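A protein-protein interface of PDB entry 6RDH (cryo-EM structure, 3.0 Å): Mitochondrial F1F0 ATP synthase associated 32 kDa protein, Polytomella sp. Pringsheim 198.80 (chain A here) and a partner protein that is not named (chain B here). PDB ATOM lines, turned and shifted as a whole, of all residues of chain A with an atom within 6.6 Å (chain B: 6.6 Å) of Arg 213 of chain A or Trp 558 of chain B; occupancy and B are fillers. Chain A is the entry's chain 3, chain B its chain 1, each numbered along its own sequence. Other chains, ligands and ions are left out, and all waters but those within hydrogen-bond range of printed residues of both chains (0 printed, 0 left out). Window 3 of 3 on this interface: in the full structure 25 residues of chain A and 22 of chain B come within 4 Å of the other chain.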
ATOM      1  N   GLU A 173       3.572  20.396 -15.925  1.00  0.00           N
ATOM      2  CA  GLU A 173       4.978  20.695 -15.745  1.00  0.00           C
ATOM      3  C   GLU A 173       5.806  19.794 -16.641  1.00  0.00           C
ATOM      4  O   GLU A 173       5.300  18.848 -17.238  1.00  0.00           O
ATOM      5  CB  GLU A 173       5.398  20.574 -14.277  1.00  0.00           C
ATOM      6  CG  GLU A 173       4.818  19.423 -13.514  1.00  0.00           C
ATOM      7  CD  GLU A 173       3.820  19.881 -12.474  1.00  0.00           C
ATOM      8  OE1 GLU A 173       3.382  21.043 -12.545  1.00  0.00           O
ATOM      9  OE2 GLU A 173       3.486  19.088 -11.571  1.00  0.00           O
ATOM     10  N   THR A 174       7.091  20.126 -16.750  1.00  0.00           N
ATOM     11  CA  THR A 174       7.977  19.443 -17.680  1.00  0.00           C
ATOM     12  C   THR A 174       8.199  17.990 -17.298  1.00  0.00           C
ATOM     13  O   THR A 174       8.364  17.152 -18.185  1.00  0.00           O
ATOM     14  CB  THR A 174       9.310  20.180 -17.752  1.00  0.00           C
ATOM     15  OG1 THR A 174       9.063  21.584 -17.804  1.00  0.00           O
ATOM     16  CG2 THR A 174      10.071  19.808 -18.991  1.00  0.00           C
ATOM     17  N   GLU A 175       8.143  17.655 -16.009  1.00  0.00           N
ATOM     18  CA  GLU A 175       8.278  16.261 -15.608  1.00  0.00           C
ATOM     19  C   GLU A 175       7.096  15.411 -16.049  1.00  0.00           C
ATOM     20  O   GLU A 175       7.232  14.189 -16.132  1.00  0.00           O
ATOM     21  CB  GLU A 175       8.433  16.148 -14.095  1.00  0.00           C
ATOM     22  CG  GLU A 175       7.204  16.567 -13.321  1.00  0.00           C
ATOM     23  CD  GLU A 175       7.347  16.386 -11.832  1.00  0.00           C
ATOM     24  OE1 GLU A 175       8.411  15.908 -11.386  1.00  0.00           O
ATOM     25  OE2 GLU A 175       6.390  16.728 -11.107  1.00  0.00           O
ATOM     26  N   ASN A 206       6.396  26.717 -17.843  1.00  0.00           N
ATOM     27  CA  ASN A 206       7.160  25.993 -16.845  1.00  0.00           C
ATOM     28  C   ASN A 206       8.455  26.731 -16.585  1.00  0.00           C
ATOM     29  O   ASN A 206       8.817  27.661 -17.304  1.00  0.00           O
ATOM     30  CB  ASN A 206       7.446  24.562 -17.288  1.00  0.00           C
ATOM     31  CG  ASN A 206       6.197  23.743 -17.423  1.00  0.00           C
ATOM     32  OD1 ASN A 206       6.123  22.832 -18.230  1.00  0.00           O
ATOM     33  ND2 ASN A 206       5.202  24.068 -16.640  1.00  0.00           N
ATOM     34  N   HIS A 207       9.152  26.318 -15.535  1.00  0.00           N
ATOM     35  CA  HIS A 207      10.382  26.992 -15.163  1.00  0.00           C
ATOM     36  C   HIS A 207      11.472  26.681 -16.171  1.00  0.00           C
ATOM     37  O   HIS A 207      11.516  25.600 -16.752  1.00  0.00           O
ATOM     38  CB  HIS A 207      10.820  26.572 -13.770  1.00  0.00           C
ATOM     39  CG  HIS A 207      11.782  27.518 -13.138  1.00  0.00           C
ATOM     40  ND1 HIS A 207      13.134  27.282 -13.092  1.00  0.00           N
ATOM     41  CD2 HIS A 207      11.591  28.713 -12.544  1.00  0.00           C
ATOM     42  CE1 HIS A 207      13.736  28.288 -12.490  1.00  0.00           C
ATOM     43  NE2 HIS A 207      12.823  29.175 -12.158  1.00  0.00           N
ATOM     44  N   TYR A 208      12.348  27.649 -16.393  1.00  0.00           N
ATOM     45  CA  TYR A 208      13.342  27.516 -17.440  1.00  0.00           C
ATOM     46  C   TYR A 208      14.506  26.627 -17.047  1.00  0.00           C
ATOM     47  O   TYR A 208      15.363  26.351 -17.890  1.00  0.00           O
ATOM     48  CB  TYR A 208      13.836  28.894 -17.854  1.00  0.00           C
ATOM     49  CG  TYR A 208      14.903  29.504 -16.995  1.00  0.00           C
ATOM     50  CD1 TYR A 208      14.637  29.927 -15.709  1.00  0.00           C
ATOM     51  CD2 TYR A 208      16.171  29.697 -17.492  1.00  0.00           C
ATOM     52  CE1 TYR A 208      15.614  30.499 -14.943  1.00  0.00           C
ATOM     53  CE2 TYR A 208      17.144  30.261 -16.732  1.00  0.00           C
ATOM     54  CZ  TYR A 208      16.865  30.660 -15.466  1.00  0.00           C
ATOM     55  OH  TYR A 208      17.864  31.228 -14.731  1.00  0.00           O
ATOM     56  N   LEU A 209      14.557  26.163 -15.803  1.00  0.00           N
ATOM     57  CA  LEU A 209      15.515  25.164 -15.368  1.00  0.00           C
ATOM     58  C   LEU A 209      14.861  23.821 -15.132  1.00  0.00           C
ATOM     59  O   LEU A 209      15.476  22.944 -14.532  1.00  0.00           O
ATOM     60  CB  LEU A 209      16.214  25.611 -14.095  1.00  0.00           C
ATOM     61  CG  LEU A 209      16.896  26.958 -14.120  1.00  0.00           C
ATOM     62  CD1 LEU A 209      17.373  27.227 -12.750  1.00  0.00           C
ATOM     63  CD2 LEU A 209      18.044  26.930 -15.071  1.00  0.00           C
ATOM     64  N   ALA A 210      13.631  23.652 -15.538  1.00  0.00           N
ATOM     65  CA  ALA A 210      13.019  22.336 -15.500  1.00  0.00           C
ATOM     66  C   ALA A 210      13.612  21.352 -16.508  1.00  0.00           C
ATOM     67  O   ALA A 210      13.545  20.145 -16.252  1.00  0.00           O
ATOM     68  CB  ALA A 210      11.510  22.456 -15.690  1.00  0.00           C
ATOM     69  N   PRO A 211      14.151  21.769 -17.667  1.00  0.00           N
ATOM     70  CA  PRO A 211      15.022  20.841 -18.399  1.00  0.00           C
ATOM     71  C   PRO A 211      16.282  20.436 -17.660  1.00  0.00           C
ATOM     72  O   PRO A 211      16.792  19.339 -17.901  1.00  0.00           O
ATOM     73  CB  PRO A 211      15.351  21.630 -19.665  1.00  0.00           C
ATOM     74  CG  PRO A 211      14.153  22.348 -19.929  1.00  0.00           C
ATOM     75  CD  PRO A 211      13.646  22.793 -18.609  1.00  0.00           C
ATOM     76  N   VAL A 212      16.812  21.282 -16.780  1.00  0.00           N
ATOM     77  CA  VAL A 212      18.013  20.923 -16.035  1.00  0.00           C
ATOM     78  C   VAL A 212      17.714  19.816 -15.025  1.00  0.00           C
ATOM     79  O   VAL A 212      18.570  18.977 -14.732  1.00  0.00           O
ATOM     80  CB  VAL A 212      18.588  22.194 -15.383  1.00  0.00           C
ATOM     81  CG1 VAL A 212      19.836  21.904 -14.633  1.00  0.00           C
ATOM     82  CG2 VAL A 212      18.867  23.233 -16.433  1.00  0.00           C
ATOM     83  N   ARG A 213      16.484  19.751 -14.532  1.00  0.00           N
ATOM     84  CA  ARG A 213      16.060  18.736 -13.582  1.00  0.00           C
ATOM     85  C   ARG A 213      15.510  17.485 -14.248  1.00  0.00           C
ATOM     86  O   ARG A 213      14.803  16.714 -13.594  1.00  0.00           O
ATOM     87  CB  ARG A 213      14.993  19.309 -12.652  1.00  0.00           C
ATOM     88  CG  ARG A 213      15.531  19.977 -11.427  1.00  0.00           C
ATOM     89  CD  ARG A 213      16.004  18.964 -10.425  1.00  0.00           C
ATOM     90  NE  ARG A 213      16.100  19.548  -9.100  1.00  0.00           N
ATOM     91  CZ  ARG A 213      17.139  20.249  -8.673  1.00  0.00           C
ATOM     92  NH1 ARG A 213      17.141  20.752  -7.451  1.00  0.00           N
ATOM     93  NH2 ARG A 213      18.181  20.443  -9.462  1.00  0.00           N
ATOM     94  N   ALA A 214      15.802  17.262 -15.522  1.00  0.00           N
ATOM     95  CA  ALA A 214      15.066  16.266 -16.290  1.00  0.00           C
ATOM     96  C   ALA A 214      15.833  14.979 -16.527  1.00  0.00           C
ATOM     97  O   ALA A 214      15.243  13.897 -16.483  1.00  0.00           O
ATOM     98  CB  ALA A 214      14.654  16.848 -17.639  1.00  0.00           C
ATOM     99  N   GLY A 215      17.124  15.060 -16.808  1.00  0.00           N
ATOM    100  CA  GLY A 215      17.840  13.872 -17.214  1.00  0.00           C
ATOM    101  C   GLY A 215      17.701  13.679 -18.706  1.00  0.00           C
ATOM    102  O   GLY A 215      16.582  13.602 -19.214  1.00  0.00           O
ATOM    103  N   GLY A 243      19.095  21.470 -20.822  1.00  0.00           N
ATOM    104  CA  GLY A 243      19.176  20.259 -20.042  1.00  0.00           C
ATOM    105  C   GLY A 243      20.260  19.291 -20.441  1.00  0.00           C
ATOM    106  O   GLY A 243      20.341  18.217 -19.844  1.00  0.00           O
ATOM    107  N   ILE B 553       3.533  32.248 -10.089  1.00  0.00           N
ATOM    108  CA  ILE B 553       3.452  31.497  -8.845  1.00  0.00           C
ATOM    109  C   ILE B 553       3.808  30.039  -9.074  1.00  0.00           C
ATOM    110  O   ILE B 553       4.468  29.422  -8.238  1.00  0.00           O
ATOM    111  CB  ILE B 553       2.047  31.692  -8.251  1.00  0.00           C
ATOM    112  CG1 ILE B 553       1.896  33.116  -7.726  1.00  0.00           C
ATOM    113  CG2 ILE B 553       1.733  30.711  -7.185  1.00  0.00           C
ATOM    114  CD1 ILE B 553       3.004  33.596  -6.855  1.00  0.00           C
ATOM    115  N   LYS B 554       3.471  29.496 -10.241  1.00  0.00           N
ATOM    116  CA  LYS B 554       3.853  28.129 -10.580  1.00  0.00           C
ATOM    117  C   LYS B 554       5.361  27.970 -10.716  1.00  0.00           C
ATOM    118  O   LYS B 554       5.936  27.002 -10.208  1.00  0.00           O
ATOM    119  CB  LYS B 554       3.160  27.722 -11.868  1.00  0.00           C
ATOM    120  CG  LYS B 554       3.611  26.426 -12.419  1.00  0.00           C
ATOM    121  CD  LYS B 554       2.902  26.117 -13.684  1.00  0.00           C
ATOM    122  CE  LYS B 554       3.177  24.714 -14.072  1.00  0.00           C
ATOM    123  NZ  LYS B 554       2.498  24.398 -15.338  1.00  0.00           N
ATOM    124  N   LYS B 555       6.025  28.926 -11.355  1.00  0.00           N
ATOM    125  CA  LYS B 555       7.472  28.842 -11.516  1.00  0.00           C
ATOM    126  C   LYS B 555       8.207  29.080 -10.204  1.00  0.00           C
ATOM    127  O   LYS B 555       9.227  28.437  -9.928  1.00  0.00           O
ATOM    128  CB  LYS B 555       7.926  29.845 -12.554  1.00  0.00           C
ATOM    129  CG  LYS B 555       7.379  29.568 -13.898  1.00  0.00           C
ATOM    130  CD  LYS B 555       7.606  30.722 -14.793  1.00  0.00           C
ATOM    131  CE  LYS B 555       6.982  30.457 -16.102  1.00  0.00           C
ATOM    132  NZ  LYS B 555       7.447  31.407 -17.114  1.00  0.00           N
ATOM    133  N   ILE B 556       7.704  29.997  -9.383  1.00  0.00           N
ATOM    134  CA  ILE B 556       8.305  30.245  -8.079  1.00  0.00           C
ATOM    135  C   ILE B 556       8.136  29.030  -7.176  1.00  0.00           C
ATOM    136  O   ILE B 556       9.059  28.644  -6.447  1.00  0.00           O
ATOM    137  CB  ILE B 556       7.689  31.519  -7.480  1.00  0.00           C
ATOM    138  CG1 ILE B 556       8.209  32.741  -8.213  1.00  0.00           C
ATOM    139  CG2 ILE B 556       7.996  31.652  -6.036  1.00  0.00           C
ATOM    140  CD1 ILE B 556       7.433  33.950  -7.936  1.00  0.00           C
ATOM    141  N   ASP B 557       6.986  28.364  -7.260  1.00  0.00           N
ATOM    142  CA  ASP B 557       6.786  27.127  -6.523  1.00  0.00           C
ATOM    143  C   ASP B 557       7.634  25.991  -7.069  1.00  0.00           C
ATOM    144  O   ASP B 557       7.955  25.063  -6.330  1.00  0.00           O
ATOM    145  CB  ASP B 557       5.318  26.744  -6.559  1.00  0.00           C
ATOM    146  CG  ASP B 557       4.474  27.651  -5.725  1.00  0.00           C
ATOM    147  OD1 ASP B 557       5.048  28.540  -5.079  1.00  0.00           O
ATOM    148  OD2 ASP B 557       3.241  27.484  -5.710  1.00  0.00           O
ATOM    149  N   TRP B 558       7.992  26.024  -8.351  1.00  0.00           N
ATOM    150  CA  TRP B 558       8.975  25.066  -8.843  1.00  0.00           C
ATOM    151  C   TRP B 558      10.329  25.308  -8.210  1.00  0.00           C
ATOM    152  O   TRP B 558      11.050  24.358  -7.903  1.00  0.00           O
ATOM    153  CB  TRP B 558       9.101  25.134 -10.362  1.00  0.00           C
ATOM    154  CG  TRP B 558       9.967  24.054 -10.924  1.00  0.00           C
ATOM    155  CD1 TRP B 558       9.558  22.851 -11.375  1.00  0.00           C
ATOM    156  CD2 TRP B 558      11.392  24.076 -11.084  1.00  0.00           C
ATOM    157  NE1 TRP B 558      10.627  22.116 -11.800  1.00  0.00           N
ATOM    158  CE2 TRP B 558      11.764  22.852 -11.628  1.00  0.00           C
ATOM    159  CE3 TRP B 558      12.385  25.015 -10.815  1.00  0.00           C
ATOM    160  CZ2 TRP B 558      13.074  22.542 -11.910  1.00  0.00           C
ATOM    161  CZ3 TRP B 558      13.679  24.700 -11.089  1.00  0.00           C
ATOM    162  CH2 TRP B 558      14.016  23.481 -11.630  1.00  0.00           C
ATOM    163  N   GLU B 559      10.716  26.569  -8.053  1.00  0.00           N
ATOM    164  CA  GLU B 559      12.000  26.860  -7.419  1.00  0.00           C
ATOM    165  C   GLU B 559      12.003  26.470  -5.950  1.00  0.00           C
ATOM    166  O   GLU B 559      13.038  26.070  -5.415  1.00  0.00           O
ATOM    167  CB  GLU B 559      12.335  28.332  -7.539  1.00  0.00           C
ATOM    168  CG  GLU B 559      12.504  28.787  -8.924  1.00  0.00           C
ATOM    169  CD  GLU B 559      13.249  30.076  -9.015  1.00  0.00           C
ATOM    170  OE1 GLU B 559      13.792  30.510  -7.990  1.00  0.00           O
ATOM    171  OE2 GLU B 559      13.297  30.661 -10.107  1.00  0.00           O
ATOM    172  N   THR B 560      10.870  26.607  -5.272  1.00  0.00           N
ATOM    173  CA  THR B 560      10.805  26.176  -3.879  1.00  0.00           C
ATOM    174  C   THR B 560      10.780  24.656  -3.772  1.00  0.00           C
ATOM    175  O   THR B 560      11.435  24.084  -2.899  1.00  0.00           O
ATOM    176  CB  THR B 560       9.588  26.788  -3.197  1.00  0.00           C
ATOM    177  OG1 THR B 560       9.622  28.207  -3.349  1.00  0.00           O
ATOM    178  CG2 THR B 560       9.588  26.481  -1.746  1.00  0.00           C
ATOM    179  N   THR B 561      10.052  23.987  -4.668  1.00  0.00           N
ATOM    180  CA  THR B 561       9.942  22.531  -4.641  1.00  0.00           C
ATOM    181  C   THR B 561      11.270  21.866  -4.950  1.00  0.00           C
ATOM    182  O   THR B 561      11.618  20.845  -4.350  1.00  0.00           O
ATOM    183  CB  THR B 561       8.892  22.071  -5.649  1.00  0.00           C
ATOM    184  OG1 THR B 561       7.716  22.866  -5.511  1.00  0.00           O
ATOM    185  CG2 THR B 561       8.517  20.645  -5.415  1.00  0.00           C
ATOM    186  N   ASN B 562      12.031  22.431  -5.878  1.00  0.00           N
ATOM    187  CA  ASN B 562      13.261  21.819  -6.348  1.00  0.00           C
ATOM    188  C   ASN B 562      14.494  22.438  -5.723  1.00  0.00           C
ATOM    189  O   ASN B 562      15.515  22.575  -6.398  1.00  0.00           O
ATOM    190  CB  ASN B 562      13.330  21.896  -7.861  1.00  0.00           C
ATOM    191  CG  ASN B 562      12.237  21.112  -8.506  1.00  0.00           C
ATOM    192  OD1 ASN B 562      11.101  21.143  -8.067  1.00  0.00           O
ATOM    193  ND2 ASN B 562      12.579  20.366  -9.530  1.00  0.00           N
ATOM    194  N   ALA B 563      14.391  22.848  -4.457  1.00  0.00           N
ATOM    195  CA  ALA B 563      15.500  23.229  -3.587  1.00  0.00           C
ATOM    196  C   ALA B 563      16.292  24.415  -4.102  1.00  0.00           C
ATOM    197  O   ALA B 563      17.450  24.592  -3.730  1.00  0.00           O
ATOM    198  CB  ALA B 563      16.438  22.049  -3.341  1.00  0.00           C
ATOM    199  N   LEU B 564      15.696  25.238  -4.946  1.00  0.00           N
ATOM    200  CA  LEU B 564      16.363  26.391  -5.521  1.00  0.00           C
ATOM    201  C   LEU B 564      15.719  27.669  -5.026  1.00  0.00           C
ATOM    202  O   LEU B 564      15.606  28.649  -5.749  1.00  0.00           O
ATOM    203  CB  LEU B 564      16.334  26.332  -7.040  1.00  0.00           C
ATOM    204  CG  LEU B 564      17.133  25.213  -7.686  1.00  0.00           C
ATOM    205  CD1 LEU B 564      16.739  25.110  -9.130  1.00  0.00           C
ATOM    206  CD2 LEU B 564      18.599  25.505  -7.556  1.00  0.00           C
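ND2 of Asn 206 of chain A sits close to NZ of Lys 554 of chain B (3.0 Å).
NE2 of His 207 of chain A lies within hydrogen-bond range of OE2 of Glu 559 of chain B (2.6 Å).
The backbone carbonyl oxygen (O) of Asn 562 of chain B sits at hydrogen-bond distance from the guanidinium group (NH1) of Arg 213 of chain A.
The side-chain amide oxygen of Asn 562 of chain B sits close to the backbone carbonyl oxygen of Trp 558 of chain B, at 3.2 Å.
The backbone NH (N) of Leu 564 of chain B is in hydrogen-bond range of the backbone carbonyl oxygen (O) of Glu 559 of chain B, 2.8 Å away.
OD1 of Asn 206 of chain A is in hydrogen-bond range of OG1 of Thr 174 of chain A (3.2 Å).
A ring nitrogen (ND1) of His 207 of chain A lies close to the backbone NH of Leu 209 of chain A, 3.3 Å away.
OE1 of Glu 173 of chain A touches CE of Lys 554 of chain B, at 3.98 Å.
Asn 206 of chain A touches Lys 555 of chain B.
Lys 555 of chain B touches His 207 of chain A (O to CD2, 3.5 Å).
Trp 558 of chain B touches His 207 of chain A.
Leu 209 of chain A touches Trp 558 of chain B.
Ala 210 of chain A touches Trp 558 of chain B (CA to CZ2, 3.6 Å).
Trp 558 of chain B touches Arg 213 of chain A (CZ2 to CG, 3.6 Å).
Arg 213 of chain A touches just these residues of chain B: Trp 558 and Asn 562.
Printed residues of chain A within 4 Å of Asn 562 of chain B: Arg 213.
Of the printed residues of chain A, Lys 555 of chain B touches Asn 206 and His 207.
Of the printed residues of chain A, Lys 554 of chain B touches Glu 173 and Asn 206.
Printed residues of chain B within 4 Å of Asn 206 of chain A: Lys 554 and Lys 555.
The nearest residue of chain B that does not touch Arg 213 of chain A is Ala 563 of chain B (4.4 Å).
Of the 12 printed residues of chain B, 5 touch a printed residue of chain A.
Hydrophobic or aromatic side chains of chain B within 4 Å of the printed part of chain A: Trp 558.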
